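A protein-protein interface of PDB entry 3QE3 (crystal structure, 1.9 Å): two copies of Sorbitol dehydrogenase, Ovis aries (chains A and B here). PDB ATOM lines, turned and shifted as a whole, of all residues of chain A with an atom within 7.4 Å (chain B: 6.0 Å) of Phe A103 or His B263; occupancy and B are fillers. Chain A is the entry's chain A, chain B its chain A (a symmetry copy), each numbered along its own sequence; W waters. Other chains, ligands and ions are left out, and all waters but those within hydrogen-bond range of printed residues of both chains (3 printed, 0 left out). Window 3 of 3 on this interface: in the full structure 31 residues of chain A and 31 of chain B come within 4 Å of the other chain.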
ATOM      1  N   GLN A  99       3.312  14.238  16.830  1.00  0.00           N
ATOM      2  CA  GLN A  99       2.667  13.333  17.778  1.00  0.00           C
ATOM      3  C   GLN A  99       1.700  14.064  18.682  1.00  0.00           C
ATOM      4  O   GLN A  99       1.890  15.238  18.990  1.00  0.00           O
ATOM      5  CB  GLN A  99       3.703  12.642  18.656  1.00  0.00           C
ATOM      6  CG  GLN A  99       4.836  11.993  17.906  1.00  0.00           C
ATOM      7  CD  GLN A  99       5.824  11.327  18.840  1.00  0.00           C
ATOM      8  OE1 GLN A  99       5.715  11.436  20.066  1.00  0.00           O
ATOM      9  NE2 GLN A  99       6.797  10.628  18.267  1.00  0.00           N
ATOM     10  N   THR A 100       0.669  13.358  19.126  1.00  0.00           N
ATOM     11  CA  THR A 100      -0.235  13.902  20.125  1.00  0.00           C
ATOM     12  C   THR A 100       0.363  13.680  21.518  1.00  0.00           C
ATOM     13  O   THR A 100      -0.145  12.876  22.287  1.00  0.00           O
ATOM     14  CB  THR A 100      -1.619  13.225  20.047  1.00  0.00           C
ATOM     15  OG1 THR A 100      -2.066  13.208  18.691  1.00  0.00           O
ATOM     16  CG2 THR A 100      -2.645  13.967  20.907  1.00  0.00           C
ATOM     17  N   ASP A 101       1.452  14.380  21.832  1.00  0.00           N
ATOM     18  CA  ASP A 101       2.089  14.229  23.136  1.00  0.00           C
ATOM     19  C   ASP A 101       1.432  15.129  24.180  1.00  0.00           C
ATOM     20  O   ASP A 101       0.451  15.815  23.888  1.00  0.00           O
ATOM     21  CB  ASP A 101       3.613  14.438  23.062  1.00  0.00           C
ATOM     22  CG  ASP A 101       4.010  15.859  22.638  1.00  0.00           C
ATOM     23  OD1 ASP A 101       3.143  16.762  22.628  1.00  0.00           O
ATOM     24  OD2 ASP A 101       5.206  16.067  22.333  1.00  0.00           O
ATOM     25  N   GLU A 102       1.943  15.117  25.403  1.00  0.00           N
ATOM     26  CA  GLU A 102       1.306  15.898  26.460  1.00  0.00           C
ATOM     27  C   GLU A 102       1.333  17.408  26.208  1.00  0.00           C
ATOM     28  O   GLU A 102       0.381  18.105  26.551  1.00  0.00           O
ATOM     29  CB  GLU A 102       1.882  15.558  27.832  1.00  0.00           C
ATOM     30  CG  GLU A 102       1.508  14.141  28.299  1.00  0.00           C
ATOM     31  CD  GLU A 102      -0.004  13.875  28.293  1.00  0.00           C
ATOM     32  OE1 GLU A 102      -0.769  14.769  28.717  1.00  0.00           O
ATOM     33  OE2 GLU A 102      -0.422  12.770  27.865  1.00  0.00           O
ATOM     34  N   PHE A 103       2.407  17.911  25.607  1.00  0.00           N
ATOM     35  CA  PHE A 103       2.485  19.343  25.289  1.00  0.00           C
ATOM     36  C   PHE A 103       1.367  19.743  24.335  1.00  0.00           C
ATOM     37  O   PHE A 103       0.766  20.814  24.468  1.00  0.00           O
ATOM     38  CB  PHE A 103       3.844  19.698  24.679  1.00  0.00           C
ATOM     39  CG  PHE A 103       4.986  19.578  25.632  1.00  0.00           C
ATOM     40  CD1 PHE A 103       5.159  20.504  26.641  1.00  0.00           C
ATOM     41  CD2 PHE A 103       5.894  18.538  25.517  1.00  0.00           C
ATOM     42  CE1 PHE A 103       6.218  20.398  27.520  1.00  0.00           C
ATOM     43  CE2 PHE A 103       6.944  18.421  26.394  1.00  0.00           C
ATOM     44  CZ  PHE A 103       7.109  19.356  27.397  1.00  0.00           C
ATOM     45  N   CYS A 104       1.111  18.888  23.353  1.00  0.00           N
ATOM     46  CA  CYS A 104       0.040  19.117  22.401  1.00  0.00           C
ATOM     47  C   CYS A 104      -1.304  19.092  23.103  1.00  0.00           C
ATOM     48  O   CYS A 104      -2.112  19.994  22.935  1.00  0.00           O
ATOM     49  CB  CYS A 104       0.078  18.079  21.273  1.00  0.00           C
ATOM     50  SG  CYS A 104       1.511  18.315  20.137  1.00  0.00           S
ATOM     51  N   LYS A 105      -1.545  18.059  23.903  1.00  0.00           N
ATOM     52  CA  LYS A 105      -2.826  17.952  24.590  1.00  0.00           C
ATOM     53  C   LYS A 105      -3.183  19.182  25.439  1.00  0.00           C
ATOM     54  O   LYS A 105      -4.335  19.631  25.439  1.00  0.00           O
ATOM     55  CB  LYS A 105      -2.874  16.683  25.434  1.00  0.00           C
ATOM     56  CG  LYS A 105      -2.815  15.405  24.635  1.00  0.00           C
ATOM     57  CD  LYS A 105      -2.956  14.219  25.586  1.00  0.00           C
ATOM     58  CE  LYS A 105      -2.571  12.928  24.943  1.00  0.00           C
ATOM     59  NZ  LYS A 105      -2.469  11.871  25.970  1.00  0.00           N
ATOM     60  N   ILE A 106      -2.208  19.719  26.167  1.00  0.00           N
ATOM     61  CA  ILE A 106      -2.473  20.880  27.029  1.00  0.00           C
ATOM     62  C   ILE A 106      -2.446  22.196  26.285  1.00  0.00           C
ATOM     63  O   ILE A 106      -2.625  23.242  26.894  1.00  0.00           O
ATOM     64  CB  ILE A 106      -1.490  21.003  28.219  1.00  0.00           C
ATOM     65  CG1 ILE A 106      -0.075  21.309  27.711  1.00  0.00           C
ATOM     66  CG2 ILE A 106      -1.523  19.740  29.062  1.00  0.00           C
ATOM     67  CD1 ILE A 106       0.880  21.716  28.798  1.00  0.00           C
ATOM     68  N   GLY A 107      -2.206  22.152  24.977  1.00  0.00           N
ATOM     69  CA  GLY A 107      -2.300  23.359  24.176  1.00  0.00           C
ATOM     70  C   GLY A 107      -1.001  24.140  24.046  1.00  0.00           C
ATOM     71  O   GLY A 107      -1.022  25.315  23.695  1.00  0.00           O
ATOM     72  N   ARG A 108       0.121  23.493  24.338  1.00  0.00           N
ATOM     73  CA  ARG A 108       1.440  24.113  24.173  1.00  0.00           C
ATOM     74  C   ARG A 108       2.309  23.338  23.187  1.00  0.00           C
ATOM     75  O   ARG A 108       3.433  22.948  23.493  1.00  0.00           O
ATOM     76  CB  ARG A 108       2.133  24.280  25.523  1.00  0.00           C
ATOM     77  CG  ARG A 108       1.304  25.119  26.513  1.00  0.00           C
ATOM     78  CD  ARG A 108       2.035  25.379  27.818  1.00  0.00           C
ATOM     79  NE  ARG A 108       3.125  26.358  27.716  1.00  0.00           N
ATOM     80  CZ  ARG A 108       3.802  26.801  28.770  1.00  0.00           C
ATOM     81  NH1 ARG A 108       3.499  26.353  29.983  1.00  0.00           N
ATOM     82  NH2 ARG A 108       4.785  27.672  28.622  1.00  0.00           N
ATOM     83  N   TYR A 109       1.792  23.150  21.978  1.00  0.00           N
ATOM     84  CA  TYR A 109       2.450  22.271  21.021  1.00  0.00           C
ATOM     85  C   TYR A 109       3.827  22.779  20.583  1.00  0.00           C
ATOM     86  O   TYR A 109       4.631  22.015  20.061  1.00  0.00           O
ATOM     87  CB  TYR A 109       1.549  21.988  19.820  1.00  0.00           C
ATOM     88  CG  TYR A 109       1.146  23.209  19.019  1.00  0.00           C
ATOM     89  CD1 TYR A 109       1.988  23.738  18.060  1.00  0.00           C
ATOM     90  CD2 TYR A 109      -0.095  23.814  19.216  1.00  0.00           C
ATOM     91  CE1 TYR A 109       1.614  24.858  17.316  1.00  0.00           C
ATOM     92  CE2 TYR A 109      -0.479  24.916  18.489  1.00  0.00           C
ATOM     93  CZ  TYR A 109       0.382  25.440  17.531  1.00  0.00           C
ATOM     94  OH  TYR A 109       0.001  26.543  16.797  1.00  0.00           O
ATOM     95  N   ASN A 110       4.107  24.059  20.825  1.00  0.00           N
ATOM     96  CA  ASN A 110       5.396  24.639  20.437  1.00  0.00           C
ATOM     97  C   ASN A 110       6.543  23.961  21.189  1.00  0.00           C
ATOM     98  O   ASN A 110       7.679  23.880  20.693  1.00  0.00           O
ATOM     99  CB  ASN A 110       5.403  26.162  20.651  1.00  0.00           C
ATOM    100  CG  ASN A 110       5.159  26.557  22.106  1.00  0.00           C
ATOM    101  OD1 ASN A 110       4.156  26.166  22.715  1.00  0.00           O
ATOM    102  ND2 ASN A 110       6.080  27.340  22.666  1.00  0.00           N
ATOM    103  N   LEU A 111       6.214  23.425  22.367  1.00  0.00           N
ATOM    104  CA  LEU A 111       7.185  22.785  23.245  1.00  0.00           C
ATOM    105  C   LEU A 111       7.353  21.291  22.987  1.00  0.00           C
ATOM    106  O   LEU A 111       8.195  20.650  23.610  1.00  0.00           O
ATOM    107  CB  LEU A 111       6.805  23.011  24.711  1.00  0.00           C
ATOM    108  CG  LEU A 111       6.775  24.474  25.175  1.00  0.00           C
ATOM    109  CD1 LEU A 111       6.341  24.505  26.659  1.00  0.00           C
ATOM    110  CD2 LEU A 111       8.134  25.089  24.975  1.00  0.00           C
ATOM    111  N   SER A 112       6.553  20.739  22.079  1.00  0.00           N
ATOM    112  CA  SER A 112       6.660  19.328  21.710  1.00  0.00           C
ATOM    113  C   SER A 112       8.056  18.980  21.177  1.00  0.00           C
ATOM    114  O   SER A 112       8.501  19.554  20.193  1.00  0.00           O
ATOM    115  CB  SER A 112       5.621  18.988  20.645  1.00  0.00           C
ATOM    116  OG  SER A 112       5.702  17.616  20.286  1.00  0.00           O
ATOM    117  N   PRO A 113       8.752  18.027  21.818  1.00  0.00           N
ATOM    118  CA  PRO A 113      10.127  17.733  21.391  1.00  0.00           C
ATOM    119  C   PRO A 113      10.246  17.103  20.003  1.00  0.00           C
ATOM    120  O   PRO A 113      11.336  17.139  19.423  1.00  0.00           O
ATOM    121  CB  PRO A 113      10.630  16.749  22.463  1.00  0.00           C
ATOM    122  CG  PRO A 113       9.404  16.167  23.061  1.00  0.00           C
ATOM    123  CD  PRO A 113       8.378  17.270  23.028  1.00  0.00           C
ATOM    124  N   THR A 114       9.161  16.546  19.471  1.00  0.00           N
ATOM    125  CA  THR A 114       9.224  15.875  18.169  1.00  0.00           C
ATOM    126  C   THR A 114       8.564  16.686  17.056  1.00  0.00           C
ATOM    127  O   THR A 114       8.315  16.178  15.971  1.00  0.00           O
ATOM    128  CB  THR A 114       8.601  14.464  18.236  1.00  0.00           C
ATOM    129  OG1 THR A 114       7.235  14.558  18.665  1.00  0.00           O
ATOM    130  CG2 THR A 114       9.384  13.572  19.219  1.00  0.00           C
ATOM    131  N   SER B 240      10.264  11.958  36.395  1.00  0.00           N
ATOM    132  CA  SER B 240      10.029  13.021  35.424  1.00  0.00           C
ATOM    133  C   SER B 240      10.636  14.324  35.923  1.00  0.00           C
ATOM    134  O   SER B 240      11.097  14.409  37.056  1.00  0.00           O
ATOM    135  CB  SER B 240       8.529  13.200  35.148  1.00  0.00           C
ATOM    136  OG  SER B 240       7.803  13.419  36.341  1.00  0.00           O
ATOM    137  N   LYS B 241      10.658  15.332  35.066  1.00  0.00           N
ATOM    138  CA  LYS B 241      11.128  16.649  35.473  1.00  0.00           C
ATOM    139  C   LYS B 241       9.994  17.329  36.227  1.00  0.00           C
ATOM    140  O   LYS B 241       8.846  17.276  35.795  1.00  0.00           O
ATOM    141  CB  LYS B 241      11.538  17.481  34.252  1.00  0.00           C
ATOM    142  CG  LYS B 241      12.825  17.028  33.568  1.00  0.00           C
ATOM    143  CD  LYS B 241      13.430  18.195  32.789  1.00  0.00           C
ATOM    144  CE  LYS B 241      14.777  17.847  32.190  1.00  0.00           C
ATOM    145  NZ  LYS B 241      14.679  16.694  31.248  1.00  0.00           N
ATOM    146  N   PRO B 242      10.310  17.959  37.362  1.00  0.00           N
ATOM    147  CA  PRO B 242       9.275  18.615  38.170  1.00  0.00           C
ATOM    148  C   PRO B 242       8.669  19.831  37.469  1.00  0.00           C
ATOM    149  O   PRO B 242       9.407  20.653  36.923  1.00  0.00           O
ATOM    150  CB  PRO B 242      10.040  19.068  39.416  1.00  0.00           C
ATOM    151  CG  PRO B 242      11.483  19.166  38.960  1.00  0.00           C
ATOM    152  CD  PRO B 242      11.642  18.031  37.989  1.00  0.00           C
ATOM    153  N   GLU B 243       7.348  19.953  37.493  1.00  0.00           N
ATOM    154  CA  GLU B 243       6.698  21.121  36.880  1.00  0.00           C
ATOM    155  C   GLU B 243       7.115  22.421  37.553  1.00  0.00           C
ATOM    156  O   GLU B 243       7.107  23.486  36.924  1.00  0.00           O
ATOM    157  CB  GLU B 243       5.169  21.005  36.917  1.00  0.00           C
ATOM    158  CG  GLU B 243       4.594  19.866  36.093  1.00  0.00           C
ATOM    159  CD  GLU B 243       4.394  18.593  36.921  1.00  0.00           C
ATOM    160  OE1 GLU B 243       4.967  18.489  38.024  1.00  0.00           O
ATOM    161  OE2 GLU B 243       3.678  17.689  36.457  1.00  0.00           O
ATOM    162  N   VAL B 244       7.448  22.337  38.838  1.00  0.00           N
ATOM    163  CA  VAL B 244       7.803  23.513  39.635  1.00  0.00           C
ATOM    164  C   VAL B 244       9.088  23.254  40.416  1.00  0.00           C
ATOM    165  O   VAL B 244       9.261  22.171  40.990  1.00  0.00           O
ATOM    166  CB  VAL B 244       6.705  23.858  40.668  1.00  0.00           C
ATOM    167  CG1 VAL B 244       7.222  24.885  41.672  1.00  0.00           C
ATOM    168  CG2 VAL B 244       5.438  24.348  39.975  1.00  0.00           C
ATOM    169  N   TYR B 260      17.971  23.740  34.992  1.00  0.00           N
ATOM    170  CA  TYR B 260      18.122  22.482  34.267  1.00  0.00           C
ATOM    171  C   TYR B 260      17.051  21.467  34.674  1.00  0.00           C
ATOM    172  O   TYR B 260      16.597  20.668  33.853  1.00  0.00           O
ATOM    173  CB  TYR B 260      19.517  21.888  34.472  1.00  0.00           C
ATOM    174  CG  TYR B 260      20.651  22.764  33.968  1.00  0.00           C
ATOM    175  CD1 TYR B 260      20.804  23.029  32.615  1.00  0.00           C
ATOM    176  CD2 TYR B 260      21.569  23.318  34.851  1.00  0.00           C
ATOM    177  CE1 TYR B 260      21.848  23.828  32.151  1.00  0.00           C
ATOM    178  CE2 TYR B 260      22.608  24.117  34.402  1.00  0.00           C
ATOM    179  CZ  TYR B 260      22.741  24.369  33.055  1.00  0.00           C
ATOM    180  OH  TYR B 260      23.774  25.164  32.625  1.00  0.00           O
ATOM    181  N   ALA B 261      16.644  21.519  35.941  1.00  0.00           N
ATOM    182  CA  ALA B 261      15.734  20.517  36.512  1.00  0.00           C
ATOM    183  C   ALA B 261      14.269  20.695  36.108  1.00  0.00           C
ATOM    184  O   ALA B 261      13.536  19.718  35.943  1.00  0.00           O
ATOM    185  CB  ALA B 261      15.869  20.496  38.044  1.00  0.00           C
ATOM    186  N   THR B 262      13.838  21.938  35.927  1.00  0.00           N
ATOM    187  CA  THR B 262      12.415  22.210  35.778  1.00  0.00           C
ATOM    188  C   THR B 262      11.852  21.762  34.422  1.00  0.00           C
ATOM    189  O   THR B 262      12.472  21.959  33.384  1.00  0.00           O
ATOM    190  CB  THR B 262      12.125  23.702  36.048  1.00  0.00           C
ATOM    191  OG1 THR B 262      12.620  24.038  37.351  1.00  0.00           O
ATOM    192  CG2 THR B 262      10.643  23.984  36.000  1.00  0.00           C
ATOM    193  N   HIS B 263      10.681  21.146  34.451  1.00  0.00           N
ATOM    194  CA  HIS B 263       9.997  20.710  33.242  1.00  0.00           C
ATOM    195  C   HIS B 263       9.786  21.895  32.287  1.00  0.00           C
ATOM    196  O   HIS B 263       9.577  23.023  32.731  1.00  0.00           O
ATOM    197  CB  HIS B 263       8.649  20.109  33.630  1.00  0.00           C
ATOM    198  CG  HIS B 263       8.028  19.274  32.558  1.00  0.00           C
ATOM    199  ND1 HIS B 263       7.234  19.806  31.564  1.00  0.00           N
ATOM    200  CD2 HIS B 263       8.073  17.941  32.327  1.00  0.00           C
ATOM    201  CE1 HIS B 263       6.822  18.838  30.766  1.00  0.00           C
ATOM    202  NE2 HIS B 263       7.318  17.696  31.206  1.00  0.00           N
ATOM    203  N   SER B 264       9.838  21.636  30.983  1.00  0.00           N
ATOM    204  CA  SER B 264       9.608  22.688  29.988  1.00  0.00           C
ATOM    205  C   SER B 264       8.200  23.211  30.197  1.00  0.00           C
ATOM    206  O   SER B 264       7.286  22.422  30.433  1.00  0.00           O
ATOM    207  CB  SER B 264       9.731  22.125  28.571  1.00  0.00           C
ATOM    208  OG  SER B 264      11.050  21.683  28.300  1.00  0.00           O
ATOM    209  N   GLY B 265       8.018  24.529  30.093  1.00  0.00           N
ATOM    210  CA  GLY B 265       6.712  25.128  30.322  1.00  0.00           C
ATOM    211  C   GLY B 265       6.459  25.389  31.798  1.00  0.00           C
ATOM    212  O   GLY B 265       5.433  25.972  32.169  1.00  0.00           O
ATOM    213  N   GLY B 266       7.409  24.979  32.637  1.00  0.00           N
ATOM    214  CA  GLY B 266       7.245  25.038  34.084  1.00  0.00           C
ATOM    215  C   GLY B 266       7.685  26.361  34.691  1.00  0.00           C
ATOM    216  O   GLY B 266       7.901  27.337  33.980  1.00  0.00           O
ATOM    217  N   THR B 267       7.844  26.380  36.009  1.00  0.00           N
ATOM    218  CA  THR B 267       8.206  27.595  36.721  1.00  0.00           C
ATOM    219  C   THR B 267       9.234  27.366  37.840  1.00  0.00           C
ATOM    220  O   THR B 267       9.087  26.470  38.681  1.00  0.00           O
ATOM    221  CB  THR B 267       6.966  28.249  37.355  1.00  0.00           C
ATOM    222  OG1 THR B 267       5.999  28.566  36.339  1.00  0.00           O
ATOM    223  CG2 THR B 267       7.360  29.506  38.103  1.00  0.00           C
ATOM    224  N   ARG B 288      12.994  26.949  26.809  1.00  0.00           N
ATOM    225  CA  ARG B 288      12.129  25.853  27.244  1.00  0.00           C
ATOM    226  C   ARG B 288      10.858  26.388  27.905  1.00  0.00           C
ATOM    227  O   ARG B 288      10.078  25.632  28.480  1.00  0.00           O
ATOM    228  CB  ARG B 288      12.882  24.926  28.206  1.00  0.00           C
ATOM    229  CG  ARG B 288      14.098  24.240  27.576  1.00  0.00           C
ATOM    230  CD  ARG B 288      14.885  23.421  28.603  1.00  0.00           C
ATOM    231  NE  ARG B 288      14.007  22.428  29.208  1.00  0.00           N
ATOM    232  CZ  ARG B 288      13.770  22.305  30.511  1.00  0.00           C
ATOM    233  NH1 ARG B 288      14.380  23.088  31.390  1.00  0.00           N
ATOM    234  NH2 ARG B 288      12.938  21.369  30.938  1.00  0.00           N
ATOM    235  N   GLU B 289      10.657  27.696  27.785  1.00  0.00           N
ATOM    236  CA  GLU B 289       9.595  28.432  28.488  1.00  0.00           C
ATOM    237  C   GLU B 289       9.483  28.045  29.966  1.00  0.00           C
ATOM    238  O   GLU B 289       8.377  27.865  30.505  1.00  0.00           O
ATOM    239  CB  GLU B 289       8.239  28.366  27.754  1.00  0.00           C
ATOM    240  CG  GLU B 289       8.300  29.015  26.348  1.00  0.00           C
ATOM    241  CD  GLU B 289       6.988  29.014  25.581  1.00  0.00           C
ATOM    242  OE1 GLU B 289       5.972  28.475  26.075  1.00  0.00           O
ATOM    243  OE2 GLU B 289       6.971  29.560  24.453  1.00  0.00           O
ATOM    244  N   VAL B 290      10.638  27.925  30.614  1.00  0.00           N
ATOM    245  CA  VAL B 290      10.673  27.854  32.083  1.00  0.00           C
ATOM    246  C   VAL B 290      10.676  29.280  32.592  1.00  0.00           C
ATOM    247  O   VAL B 290      11.637  30.024  32.370  1.00  0.00           O
ATOM    248  CB  VAL B 290      11.938  27.125  32.601  1.00  0.00           C
ATOM    249  CG1 VAL B 290      11.951  27.047  34.138  1.00  0.00           C
ATOM    250  CG2 VAL B 290      12.047  25.722  31.991  1.00  0.00           C
HETATM  251  O   HOH W   1       3.667  27.543  25.036  1.00  0.00           O
HETATM  252  O   HOH W   2      10.365  20.773  25.229  1.00  0.00           O
HETATM  253  O   HOH W   3       5.918  28.872  30.667  1.00  0.00           O
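NH2 of Arg A108 is in salt-bridge range of OE1 of Glu B289 (2.9 Å).
The side-chain amide nitrogen (ND2) of Asn A110 is in hydrogen-bond range of the side-chain carboxylate (OE2) of Glu B289, at 3.0 Å.
NH1 of Arg A108 lies within hydrogen-bond range of O of Gly B265 (2.9 Å).
The backbone carbonyl oxygen of Glu B289 lies close to the backbone NH of Gly B265 (3.4 Å).
The backbone NH of Phe A103 sits close to the side-chain carboxylate of Asp A101, 3.3 Å away.
The side-chain amide oxygen (OD1) of Asn A110 lies close to the backbone carbonyl oxygen (O) of Arg A108 (3.4 Å).
The backbone carbonyl oxygen of Phe A103 is in hydrogen-bond range of the backbone NH of Arg A108, 2.8 Å away.
The backbone NH (N) of Gly B265 is in hydrogen-bond range of the backbone carbonyl oxygen (O) of Arg B288, 2.8 Å away.
The side-chain hydroxyl of Ser B264 lies within hydrogen-bond range of the guanidinium group of Arg B288 (3.2 Å).
Among the printed residues, merely in contact across the chains: Phe A103 with His B263 (3.4 Å), Phe A103 with Ser B264 (3.7 Å) and Leu A111 with Gly B265 (3.7 Å).
Phe A103 touches two residues of chain B.
Of the printed residues of chain A, Ser B264 touches Phe A103 (3.7 Å).
Of the printed residues of chain B, Leu A111 touches Gly B265 (3.7 Å).
Printed residues of chain B within 4 Å of Asn A110: Glu B289.
Thr A114 touches none of the printed residues of chain B.
The nearest printed residue of chain B that does not touch Arg A108 is Gly B266 (4.9 Å).
Of the 16 printed residues of chain B, 4 touch a printed residue of chain A.
Along chain B the printed residues that touch a printed residue of chain A span positions 263 to 289.
Printed residues of chain A that touch a printed residue of chain B: Phe A103, Arg A108, Asn A110 and Leu A111.
Hydrophobic or aromatic side chains of chain A within 4 Å of the printed part of chain B: Phe A103 and Leu A111.
Among the printed residues, Asp or Glu carboxylates within 4 Å of a Lys or Arg side-chain nitrogen of the other chain: Arg A108 with Glu B289.
No position is printed for both chains.
Of the 6 pairs that touch across the chains among the printed residues, none has its exchanged pair printed and touching as well.
Water W3 lies within hydrogen-bond range of NH2 of Arg A108 (2.6 Å), O of Glu B289 (2.7 Å) and O of Gly B265 (3.3 Å).
Water W1 lies within hydrogen-bond range of OE1 of Glu B289, OD1 of Asn A110 and NE of Arg A108.
Water W2 lies within hydrogen-bond range of the backbone carbonyl oxygen (O) of Leu A111 (2.7 Å) and the side-chain hydroxyl (OG) of Ser B264 (3.3 Å).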
